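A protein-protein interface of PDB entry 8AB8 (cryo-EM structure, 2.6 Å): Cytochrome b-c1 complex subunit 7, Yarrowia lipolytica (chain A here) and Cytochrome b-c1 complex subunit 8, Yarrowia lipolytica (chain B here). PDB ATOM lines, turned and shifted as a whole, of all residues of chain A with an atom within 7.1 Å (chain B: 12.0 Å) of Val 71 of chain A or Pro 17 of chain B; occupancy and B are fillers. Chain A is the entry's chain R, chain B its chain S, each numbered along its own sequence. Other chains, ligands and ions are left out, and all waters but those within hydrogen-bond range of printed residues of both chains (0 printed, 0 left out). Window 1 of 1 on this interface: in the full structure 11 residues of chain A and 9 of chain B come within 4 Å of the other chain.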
ATOM      1  N   ASP A  46      15.050   2.956 -21.640  1.00  0.00           N
ATOM      2  CA  ASP A  46      14.245   1.766 -21.407  1.00  0.00           C
ATOM      3  C   ASP A  46      12.960   1.780 -22.234  1.00  0.00           C
ATOM      4  O   ASP A  46      12.353   0.731 -22.440  1.00  0.00           O
ATOM      5  CB  ASP A  46      13.882   1.586 -19.938  1.00  0.00           C
ATOM      6  CG  ASP A  46      15.072   1.504 -19.002  1.00  0.00           C
ATOM      7  OD1 ASP A  46      16.123   0.984 -19.426  1.00  0.00           O
ATOM      8  OD2 ASP A  46      14.937   1.965 -17.851  1.00  0.00           O
ATOM      9  N   GLU A  50      11.919  -2.160 -28.917  1.00  0.00           N
ATOM     10  CA  GLU A  50      13.030  -3.078 -29.095  1.00  0.00           C
ATOM     11  C   GLU A  50      12.738  -4.188 -30.107  1.00  0.00           C
ATOM     12  O   GLU A  50      13.639  -4.974 -30.393  1.00  0.00           O
ATOM     13  CB  GLU A  50      13.423  -3.680 -27.752  1.00  0.00           C
ATOM     14  CG  GLU A  50      12.379  -4.677 -27.307  1.00  0.00           C
ATOM     15  CD  GLU A  50      12.811  -5.610 -26.199  1.00  0.00           C
ATOM     16  OE1 GLU A  50      12.977  -6.813 -26.487  1.00  0.00           O
ATOM     17  OE2 GLU A  50      12.980  -5.140 -25.054  1.00  0.00           O
ATOM     18  N   LEU A  59      20.827  -4.644 -28.108  1.00  0.00           N
ATOM     19  CA  LEU A  59      20.612  -5.074 -26.735  1.00  0.00           C
ATOM     20  C   LEU A  59      21.560  -6.214 -26.383  1.00  0.00           C
ATOM     21  O   LEU A  59      22.005  -6.295 -25.243  1.00  0.00           O
ATOM     22  CB  LEU A  59      19.149  -5.458 -26.496  1.00  0.00           C
ATOM     23  CG  LEU A  59      18.163  -4.291 -26.391  1.00  0.00           C
ATOM     24  CD1 LEU A  59      16.716  -4.765 -26.463  1.00  0.00           C
ATOM     25  CD2 LEU A  59      18.397  -3.464 -25.139  1.00  0.00           C
ATOM     26  N   THR A  65      26.290  -6.254 -17.016  1.00  0.00           N
ATOM     27  CA  THR A  65      25.814  -5.469 -15.891  1.00  0.00           C
ATOM     28  C   THR A  65      24.657  -4.552 -16.289  1.00  0.00           C
ATOM     29  O   THR A  65      23.617  -4.535 -15.625  1.00  0.00           O
ATOM     30  CB  THR A  65      26.991  -4.704 -15.279  1.00  0.00           C
ATOM     31  OG1 THR A  65      27.759  -5.700 -14.609  1.00  0.00           O
ATOM     32  CG2 THR A  65      26.586  -3.619 -14.307  1.00  0.00           C
ATOM     33  N   GLU A  66      24.861  -3.774 -17.357  1.00  0.00           N
ATOM     34  CA  GLU A  66      23.829  -2.889 -17.869  1.00  0.00           C
ATOM     35  C   GLU A  66      22.599  -3.709 -18.246  1.00  0.00           C
ATOM     36  O   GLU A  66      21.470  -3.272 -18.049  1.00  0.00           O
ATOM     37  CB  GLU A  66      24.325  -2.118 -19.092  1.00  0.00           C
ATOM     38  CG  GLU A  66      25.438  -1.132 -18.799  1.00  0.00           C
ATOM     39  CD  GLU A  66      24.997   0.273 -18.419  1.00  0.00           C
ATOM     40  OE1 GLU A  66      25.760   1.225 -18.707  1.00  0.00           O
ATOM     41  OE2 GLU A  66      23.909   0.420 -17.822  1.00  0.00           O
ATOM     42  N   SER A  67      22.841  -4.894 -18.802  1.00  0.00           N
ATOM     43  CA  SER A  67      21.754  -5.722 -19.272  1.00  0.00           C
ATOM     44  C   SER A  67      20.930  -6.229 -18.093  1.00  0.00           C
ATOM     45  O   SER A  67      19.702  -6.184 -18.152  1.00  0.00           O
ATOM     46  CB  SER A  67      22.262  -6.826 -20.118  1.00  0.00           C
ATOM     47  OG  SER A  67      21.177  -7.543 -20.677  1.00  0.00           O
ATOM     48  N   TYR A  68      21.603  -6.668 -17.022  1.00  0.00           N
ATOM     49  CA  TYR A  68      20.894  -7.177 -15.858  1.00  0.00           C
ATOM     50  C   TYR A  68      20.106  -6.061 -15.193  1.00  0.00           C
ATOM     51  O   TYR A  68      19.006  -6.311 -14.712  1.00  0.00           O
ATOM     52  CB  TYR A  68      21.839  -7.752 -14.810  1.00  0.00           C
ATOM     53  CG  TYR A  68      22.513  -9.023 -15.230  1.00  0.00           C
ATOM     54  CD1 TYR A  68      21.784 -10.083 -15.753  1.00  0.00           C
ATOM     55  CD2 TYR A  68      23.885  -9.171 -15.087  1.00  0.00           C
ATOM     56  CE1 TYR A  68      22.402 -11.269 -16.124  1.00  0.00           C
ATOM     57  CE2 TYR A  68      24.518 -10.348 -15.454  1.00  0.00           C
ATOM     58  CZ  TYR A  68      23.773 -11.396 -15.974  1.00  0.00           C
ATOM     59  OH  TYR A  68      24.404 -12.547 -16.337  1.00  0.00           O
ATOM     60  N   ASP A  69      20.658  -4.845 -15.186  1.00  0.00           N
ATOM     61  CA  ASP A  69      19.968  -3.760 -14.514  1.00  0.00           C
ATOM     62  C   ASP A  69      18.730  -3.342 -15.300  1.00  0.00           C
ATOM     63  O   ASP A  69      17.741  -2.895 -14.721  1.00  0.00           O
ATOM     64  CB  ASP A  69      20.872  -2.549 -14.330  1.00  0.00           C
ATOM     65  CG  ASP A  69      22.022  -2.760 -13.360  1.00  0.00           C
ATOM     66  OD1 ASP A  69      22.034  -3.790 -12.640  1.00  0.00           O
ATOM     67  OD2 ASP A  69      22.910  -1.882 -13.326  1.00  0.00           O
ATOM     68  N   ARG A  70      18.817  -3.414 -16.624  1.00  0.00           N
ATOM     69  CA  ARG A  70      17.686  -3.046 -17.451  1.00  0.00           C
ATOM     70  C   ARG A  70      16.553  -4.040 -17.206  1.00  0.00           C
ATOM     71  O   ARG A  70      15.406  -3.641 -17.045  1.00  0.00           O
ATOM     72  CB  ARG A  70      18.140  -3.005 -18.911  1.00  0.00           C
ATOM     73  CG  ARG A  70      17.013  -2.800 -19.912  1.00  0.00           C
ATOM     74  CD  ARG A  70      17.490  -2.664 -21.346  1.00  0.00           C
ATOM     75  NE  ARG A  70      16.372  -2.631 -22.282  1.00  0.00           N
ATOM     76  CZ  ARG A  70      15.716  -3.706 -22.712  1.00  0.00           C
ATOM     77  NH1 ARG A  70      14.715  -3.561 -23.564  1.00  0.00           N
ATOM     78  NH2 ARG A  70      16.071  -4.917 -22.313  1.00  0.00           N
ATOM     79  N   VAL A  71      16.879  -5.332 -17.145  1.00  0.00           N
ATOM     80  CA  VAL A  71      15.862  -6.335 -16.874  1.00  0.00           C
ATOM     81  C   VAL A  71      15.156  -5.999 -15.563  1.00  0.00           C
ATOM     82  O   VAL A  71      13.935  -6.048 -15.482  1.00  0.00           O
ATOM     83  CB  VAL A  71      16.460  -7.752 -16.841  1.00  0.00           C
ATOM     84  CG1 VAL A  71      15.515  -8.764 -16.202  1.00  0.00           C
ATOM     85  CG2 VAL A  71      16.876  -8.201 -18.231  1.00  0.00           C
ATOM     86  N   TYR A  72      15.926  -5.633 -14.544  1.00  0.00           N
ATOM     87  CA  TYR A  72      15.291  -5.313 -13.283  1.00  0.00           C
ATOM     88  C   TYR A  72      14.384  -4.086 -13.379  1.00  0.00           C
ATOM     89  O   TYR A  72      13.292  -4.102 -12.821  1.00  0.00           O
ATOM     90  CB  TYR A  72      16.319  -5.143 -12.173  1.00  0.00           C
ATOM     91  CG  TYR A  72      15.690  -4.674 -10.890  1.00  0.00           C
ATOM     92  CD1 TYR A  72      14.782  -5.478 -10.215  1.00  0.00           C
ATOM     93  CD2 TYR A  72      15.965  -3.418 -10.366  1.00  0.00           C
ATOM     94  CE1 TYR A  72      14.177  -5.057  -9.042  1.00  0.00           C
ATOM     95  CE2 TYR A  72      15.382  -2.988  -9.181  1.00  0.00           C
ATOM     96  CZ  TYR A  72      14.486  -3.813  -8.520  1.00  0.00           C
ATOM     97  OH  TYR A  72      13.895  -3.434  -7.351  1.00  0.00           O
ATOM     98  N   ARG A  73      14.827  -3.026 -14.058  1.00  0.00           N
ATOM     99  CA  ARG A  73      13.989  -1.839 -14.163  1.00  0.00           C
ATOM    100  C   ARG A  73      12.700  -2.159 -14.919  1.00  0.00           C
ATOM    101  O   ARG A  73      11.654  -1.622 -14.581  1.00  0.00           O
ATOM    102  CB  ARG A  73      14.714  -0.662 -14.820  1.00  0.00           C
ATOM    103  CG  ARG A  73      15.768   0.019 -13.954  1.00  0.00           C
ATOM    104  CD  ARG A  73      16.352   1.267 -14.606  1.00  0.00           C
ATOM    105  NE  ARG A  73      16.769   1.096 -15.994  1.00  0.00           N
ATOM    106  CZ  ARG A  73      17.963   0.662 -16.391  1.00  0.00           C
ATOM    107  NH1 ARG A  73      18.221   0.518 -17.680  1.00  0.00           N
ATOM    108  NH2 ARG A  73      18.892   0.358 -15.505  1.00  0.00           N
ATOM    109  N   LEU A  74      12.753  -3.043 -15.918  1.00  0.00           N
ATOM    110  CA  LEU A  74      11.537  -3.374 -16.644  1.00  0.00           C
ATOM    111  C   LEU A  74      10.577  -4.148 -15.753  1.00  0.00           C
ATOM    112  O   LEU A  74       9.375  -3.876 -15.773  1.00  0.00           O
ATOM    113  CB  LEU A  74      11.854  -4.169 -17.909  1.00  0.00           C
ATOM    114  CG  LEU A  74      12.696  -3.453 -18.961  1.00  0.00           C
ATOM    115  CD1 LEU A  74      12.868  -4.341 -20.181  1.00  0.00           C
ATOM    116  CD2 LEU A  74      12.100  -2.104 -19.345  1.00  0.00           C
ATOM    117  N   ILE A  75      11.114  -5.083 -14.965  1.00  0.00           N
ATOM    118  CA  ILE A  75      10.262  -5.890 -14.110  1.00  0.00           C
ATOM    119  C   ILE A  75       9.679  -5.007 -13.016  1.00  0.00           C
ATOM    120  O   ILE A  75       8.493  -5.076 -12.725  1.00  0.00           O
ATOM    121  CB  ILE A  75      11.014  -7.106 -13.545  1.00  0.00           C
ATOM    122  CG1 ILE A  75      11.235  -8.143 -14.646  1.00  0.00           C
ATOM    123  CG2 ILE A  75      10.286  -7.706 -12.352  1.00  0.00           C
ATOM    124  CD1 ILE A  75      12.305  -9.160 -14.316  1.00  0.00           C
ATOM    125  N   ARG A  76      10.515  -4.163 -12.425  1.00  0.00           N
ATOM    126  CA  ARG A  76      10.038  -3.271 -11.391  1.00  0.00           C
ATOM    127  C   ARG A  76       8.933  -2.345 -11.921  1.00  0.00           C
ATOM    128  O   ARG A  76       7.951  -2.117 -11.226  1.00  0.00           O
ATOM    129  CB  ARG A  76      11.250  -2.525 -10.848  1.00  0.00           C
ATOM    130  CG  ARG A  76      10.956  -1.672  -9.632  1.00  0.00           C
ATOM    131  CD  ARG A  76      11.639  -0.348  -9.880  1.00  0.00           C
ATOM    132  NE  ARG A  76      12.949  -0.099  -9.358  1.00  0.00           N
ATOM    133  CZ  ARG A  76      13.828   0.755  -9.857  1.00  0.00           C
ATOM    134  NH1 ARG A  76      14.917   0.972  -9.147  1.00  0.00           N
ATOM    135  NH2 ARG A  76      13.666   1.324 -11.043  1.00  0.00           N
ATOM    136  N   ALA A  77       9.112  -1.773 -13.118  1.00  0.00           N
ATOM    137  CA  ALA A  77       8.130  -0.846 -13.663  1.00  0.00           C
ATOM    138  C   ALA A  77       6.836  -1.579 -13.971  1.00  0.00           C
ATOM    139  O   ALA A  77       5.766  -1.022 -13.758  1.00  0.00           O
ATOM    140  CB  ALA A  77       8.634  -0.119 -14.884  1.00  0.00           C
ATOM    141  N   TYR B   7       9.307 -12.618 -32.032  1.00  0.00           N
ATOM    142  CA  TYR B   7       9.625 -11.692 -30.860  1.00  0.00           C
ATOM    143  C   TYR B   7       9.023 -12.151 -29.537  1.00  0.00           C
ATOM    144  O   TYR B   7       9.214 -11.500 -28.512  1.00  0.00           O
ATOM    145  CB  TYR B   7       9.177 -10.249 -31.103  1.00  0.00           C
ATOM    146  CG  TYR B   7      10.006  -9.562 -32.149  1.00  0.00           C
ATOM    147  CD1 TYR B   7      11.347  -9.264 -31.929  1.00  0.00           C
ATOM    148  CD2 TYR B   7       9.464  -9.271 -33.396  1.00  0.00           C
ATOM    149  CE1 TYR B   7      12.126  -8.684 -32.919  1.00  0.00           C
ATOM    150  CE2 TYR B   7      10.229  -8.685 -34.393  1.00  0.00           C
ATOM    151  CZ  TYR B   7      11.563  -8.391 -34.153  1.00  0.00           C
ATOM    152  OH  TYR B   7      12.317  -7.810 -35.131  1.00  0.00           O
ATOM    153  N   MET B   8       8.270 -13.244 -29.548  1.00  0.00           N
ATOM    154  CA  MET B   8       7.939 -13.874 -28.287  1.00  0.00           C
ATOM    155  C   MET B   8       8.213 -15.358 -28.447  1.00  0.00           C
ATOM    156  O   MET B   8       7.876 -15.919 -29.485  1.00  0.00           O
ATOM    157  CB  MET B   8       6.468 -13.655 -27.948  1.00  0.00           C
ATOM    158  CG  MET B   8       6.074 -14.322 -26.649  1.00  0.00           C
ATOM    159  SD  MET B   8       4.338 -14.053 -26.236  1.00  0.00           S
ATOM    160  CE  MET B   8       3.542 -15.294 -27.257  1.00  0.00           C
ATOM    161  N   GLY B   9       8.823 -15.979 -27.432  1.00  0.00           N
ATOM    162  CA  GLY B   9       9.015 -17.415 -27.479  1.00  0.00           C
ATOM    163  C   GLY B   9       7.883 -18.110 -26.746  1.00  0.00           C
ATOM    164  O   GLY B   9       6.716 -17.894 -27.046  1.00  0.00           O
ATOM    165  N   TRP B  10       8.257 -18.946 -25.781  1.00  0.00           N
ATOM    166  CA  TRP B  10       7.284 -19.682 -24.994  1.00  0.00           C
ATOM    167  C   TRP B  10       7.894 -19.953 -23.626  1.00  0.00           C
ATOM    168  O   TRP B  10       9.046 -19.605 -23.414  1.00  0.00           O
ATOM    169  CB  TRP B  10       6.885 -20.972 -25.715  1.00  0.00           C
ATOM    170  CG  TRP B  10       5.532 -21.451 -25.291  1.00  0.00           C
ATOM    171  CD1 TRP B  10       5.243 -22.521 -24.489  1.00  0.00           C
ATOM    172  CD2 TRP B  10       4.272 -20.847 -25.625  1.00  0.00           C
ATOM    173  NE1 TRP B  10       3.888 -22.630 -24.314  1.00  0.00           N
ATOM    174  CE2 TRP B  10       3.267 -21.618 -24.998  1.00  0.00           C
ATOM    175  CE3 TRP B  10       3.897 -19.735 -26.394  1.00  0.00           C
ATOM    176  CZ2 TRP B  10       1.910 -21.311 -25.125  1.00  0.00           C
ATOM    177  CZ3 TRP B  10       2.555 -19.438 -26.524  1.00  0.00           C
ATOM    178  CH2 TRP B  10       1.578 -20.219 -25.902  1.00  0.00           C
ATOM    179  N   GLY B  12       9.979 -21.070 -20.711  1.00  0.00           N
ATOM    180  CA  GLY B  12      11.303 -21.659 -20.743  1.00  0.00           C
ATOM    181  C   GLY B  12      12.239 -20.917 -21.693  1.00  0.00           C
ATOM    182  O   GLY B  12      13.451 -20.910 -21.476  1.00  0.00           O
ATOM    183  N   HIS B  13      11.686 -20.297 -22.739  1.00  0.00           N
ATOM    184  CA  HIS B  13      12.501 -19.601 -23.718  1.00  0.00           C
ATOM    185  C   HIS B  13      11.715 -18.401 -24.238  1.00  0.00           C
ATOM    186  O   HIS B  13      11.476 -18.271 -25.435  1.00  0.00           O
ATOM    187  CB  HIS B  13      12.971 -20.588 -24.801  1.00  0.00           C
ATOM    188  CG  HIS B  13      11.860 -21.272 -25.523  1.00  0.00           C
ATOM    189  ND1 HIS B  13      11.173 -22.335 -24.977  1.00  0.00           N
ATOM    190  CD2 HIS B  13      11.301 -21.042 -26.733  1.00  0.00           C
ATOM    191  CE1 HIS B  13      10.241 -22.737 -25.819  1.00  0.00           C
ATOM    192  NE2 HIS B  13      10.289 -21.951 -26.900  1.00  0.00           N
ATOM    193  N   MET B  14      11.304 -17.524 -23.321  1.00  0.00           N
ATOM    194  CA  MET B  14      10.379 -16.464 -23.683  1.00  0.00           C
ATOM    195  C   MET B  14      11.050 -15.414 -24.570  1.00  0.00           C
ATOM    196  O   MET B  14      10.374 -14.781 -25.372  1.00  0.00           O
ATOM    197  CB  MET B  14       9.782 -15.785 -22.448  1.00  0.00           C
ATOM    198  CG  MET B  14       8.474 -15.056 -22.729  1.00  0.00           C
ATOM    199  SD  MET B  14       7.101 -16.170 -23.162  1.00  0.00           S
ATOM    200  CE  MET B  14       6.958 -17.117 -21.646  1.00  0.00           C
ATOM    201  N   GLY B  15      12.369 -15.235 -24.436  1.00  0.00           N
ATOM    202  CA  GLY B  15      13.071 -14.216 -25.205  1.00  0.00           C
ATOM    203  C   GLY B  15      13.514 -13.018 -24.362  1.00  0.00           C
ATOM    204  O   GLY B  15      13.973 -12.012 -24.900  1.00  0.00           O
ATOM    205  N   SER B  16      13.383 -13.139 -23.038  1.00  0.00           N
ATOM    206  CA  SER B  16      13.982 -12.212 -22.092  1.00  0.00           C
ATOM    207  C   SER B  16      15.502 -12.227 -22.244  1.00  0.00           C
ATOM    208  O   SER B  16      16.091 -13.280 -22.486  1.00  0.00           O
ATOM    209  CB  SER B  16      13.580 -12.596 -20.688  1.00  0.00           C
ATOM    210  OG  SER B  16      14.254 -11.813 -19.715  1.00  0.00           O
ATOM    211  N   PRO B  17      16.202 -11.086 -22.058  1.00  0.00           N
ATOM    212  CA  PRO B  17      17.647 -11.128 -21.833  1.00  0.00           C
ATOM    213  C   PRO B  17      17.862 -11.949 -20.565  1.00  0.00           C
ATOM    214  O   PRO B  17      16.935 -12.094 -19.766  1.00  0.00           O
ATOM    215  CB  PRO B  17      18.005  -9.680 -21.506  1.00  0.00           C
ATOM    216  CG  PRO B  17      16.886  -8.875 -22.115  1.00  0.00           C
ATOM    217  CD  PRO B  17      15.646  -9.728 -21.992  1.00  0.00           C
ATOM    218  N   PRO B  18      19.060 -12.533 -20.341  1.00  0.00           N
ATOM    219  CA  PRO B  18      19.294 -13.355 -19.153  1.00  0.00           C
ATOM    220  C   PRO B  18      18.970 -12.584 -17.882  1.00  0.00           C
ATOM    221  O   PRO B  18      19.341 -11.422 -17.744  1.00  0.00           O
ATOM    222  CB  PRO B  18      20.802 -13.591 -19.194  1.00  0.00           C
ATOM    223  CG  PRO B  18      21.129 -13.536 -20.664  1.00  0.00           C
ATOM    224  CD  PRO B  18      20.239 -12.444 -21.215  1.00  0.00           C
ATOM    225  N   GLN B  19      18.246 -13.231 -16.975  1.00  0.00           N
ATOM    226  CA  GLN B  19      17.911 -12.588 -15.718  1.00  0.00           C
ATOM    227  C   GLN B  19      18.808 -13.175 -14.643  1.00  0.00           C
ATOM    228  O   GLN B  19      19.022 -14.387 -14.607  1.00  0.00           O
ATOM    229  CB  GLN B  19      16.443 -12.818 -15.375  1.00  0.00           C
ATOM    230  CG  GLN B  19      15.500 -12.456 -16.504  1.00  0.00           C
ATOM    231  CD  GLN B  19      14.064 -12.352 -16.047  1.00  0.00           C
ATOM    232  OE1 GLN B  19      13.730 -12.598 -14.887  1.00  0.00           O
ATOM    233  NE2 GLN B  19      13.194 -11.964 -16.966  1.00  0.00           N
ATOM    234  N   LYS B  20      19.355 -12.295 -13.809  1.00  0.00           N
ATOM    235  CA  LYS B  20      20.148 -12.719 -12.675  1.00  0.00           C
ATOM    236  C   LYS B  20      20.102 -11.622 -11.618  1.00  0.00           C
ATOM    237  O   LYS B  20      20.087 -10.441 -11.954  1.00  0.00           O
ATOM    238  CB  LYS B  20      21.585 -12.987 -13.120  1.00  0.00           C
ATOM    239  CG  LYS B  20      22.452 -13.662 -12.076  1.00  0.00           C
ATOM    240  CD  LYS B  20      23.759 -14.142 -12.642  1.00  0.00           C
ATOM    241  CE  LYS B  20      24.694 -14.643 -11.563  1.00  0.00           C
ATOM    242  NZ  LYS B  20      26.054 -14.893 -12.096  1.00  0.00           N
ATOM    243  N   GLY B  21      20.068 -12.029 -10.347  1.00  0.00           N
ATOM    244  CA  GLY B  21      20.207 -11.087  -9.254  1.00  0.00           C
ATOM    245  C   GLY B  21      18.880 -10.599  -8.682  1.00  0.00           C
ATOM    246  O   GLY B  21      18.891  -9.869  -7.692  1.00  0.00           O
ATOM    247  N   ILE B  22      17.748 -11.011  -9.267  1.00  0.00           N
ATOM    248  CA  ILE B  22      16.460 -10.589  -8.739  1.00  0.00           C
ATOM    249  C   ILE B  22      15.849 -11.729  -7.935  1.00  0.00           C
ATOM    250  O   ILE B  22      15.669 -12.818  -8.466  1.00  0.00           O
ATOM    251  CB  ILE B  22      15.518 -10.175  -9.882  1.00  0.00           C
ATOM    252  CG1 ILE B  22      16.139  -9.133 -10.812  1.00  0.00           C
ATOM    253  CG2 ILE B  22      14.164  -9.731  -9.336  1.00  0.00           C
ATOM    254  CD1 ILE B  22      15.481  -9.068 -12.179  1.00  0.00           C
ATOM    255  N   ALA B  23      15.488 -11.475  -6.679  1.00  0.00           N
ATOM    256  CA  ALA B  23      14.715 -12.447  -5.925  1.00  0.00           C
ATOM    257  C   ALA B  23      13.285 -11.931  -5.829  1.00  0.00           C
ATOM    258  O   ALA B  23      13.087 -10.769  -5.486  1.00  0.00           O
ATOM    259  CB  ALA B  23      15.328 -12.614  -4.562  1.00  0.00           C
ATOM    260  N   GLY B  24      12.299 -12.774  -6.149  1.00  0.00           N
ATOM    261  CA  GLY B  24      10.900 -12.379  -6.071  1.00  0.00           C
ATOM    262  C   GLY B  24      10.191 -13.123  -4.946  1.00  0.00           C
ATOM    263  O   GLY B  24      10.473 -14.292  -4.716  1.00  0.00           O
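Of the 17 printed residues of chain B, 5 touch a printed residue of chain A. Hydrophobic or aromatic side chains of chain B that line the printed part of chain A: Pro 17 and Ile 22. Of the 16 printed residues of chain A, 5 touch a printed residue of chain B. Hydrophobic or aromatic side chains of chain A that line the printed part of chain B: Tyr 68, Val 71, Tyr 72 and Ile 75. Among the printed residues, no Asp or Glu carboxylate lies within 4 Å of a Lys or Arg side-chain nitrogen of the other chain.
Val 71 of chain A touches just these residues of chain B: Pro 17 and Gln 19. No residue of chain B comes within 4 Å of Asp 69 of chain A. No residue of chain B comes within 4 Å of Arg 70 of chain A. No residue of chain B comes within 4 Å of Arg 73 of chain A. No residue of chain B comes within 4 Å of Leu 74 of chain A. Of chain B, only Gln 19 (3.8 Å) and Ile 22 (3.8 Å) come within 4 Å of Ile 75 of chain A. Printed residues of chain B within 4 Å of Tyr 72 of chain A: Ile 22. Of the printed residues of chain A, Gln 19 of chain B touches Val 71 (3.7 Å) and Ile 75 (3.8 Å). The nearest residue of chain A that does not touch Pro 17 of chain B is Arg 70 of chain A (4.05 Å).
OG of Ser 16 of chain B lies within hydrogen-bond range of NE2 of Gln 19 of chain B, at 3.0 Å.
OG of Ser 67 of chain A touches CB of Pro 17 of chain B, 3.9 Å away. CD1 of Tyr 68 of chain A touches O of Pro 18 of chain B, at 3.4 Å. Lys 20 of chain B touches Tyr 68 of chain A. CG2 of Val 71 of chain A touches CB of Pro 17 of chain B, 3.8 Å away. Val 71 of chain A touches Gln 19 of chain B. Tyr 72 of chain A touches Ile 22 of chain B (CA to CD1, 3.9 Å). Gln 19 of chain B touches Ile 75 of chain A. CD1 of Ile 75 of chain A touches CD1 of Ile 22 of chain B (3.8 Å).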
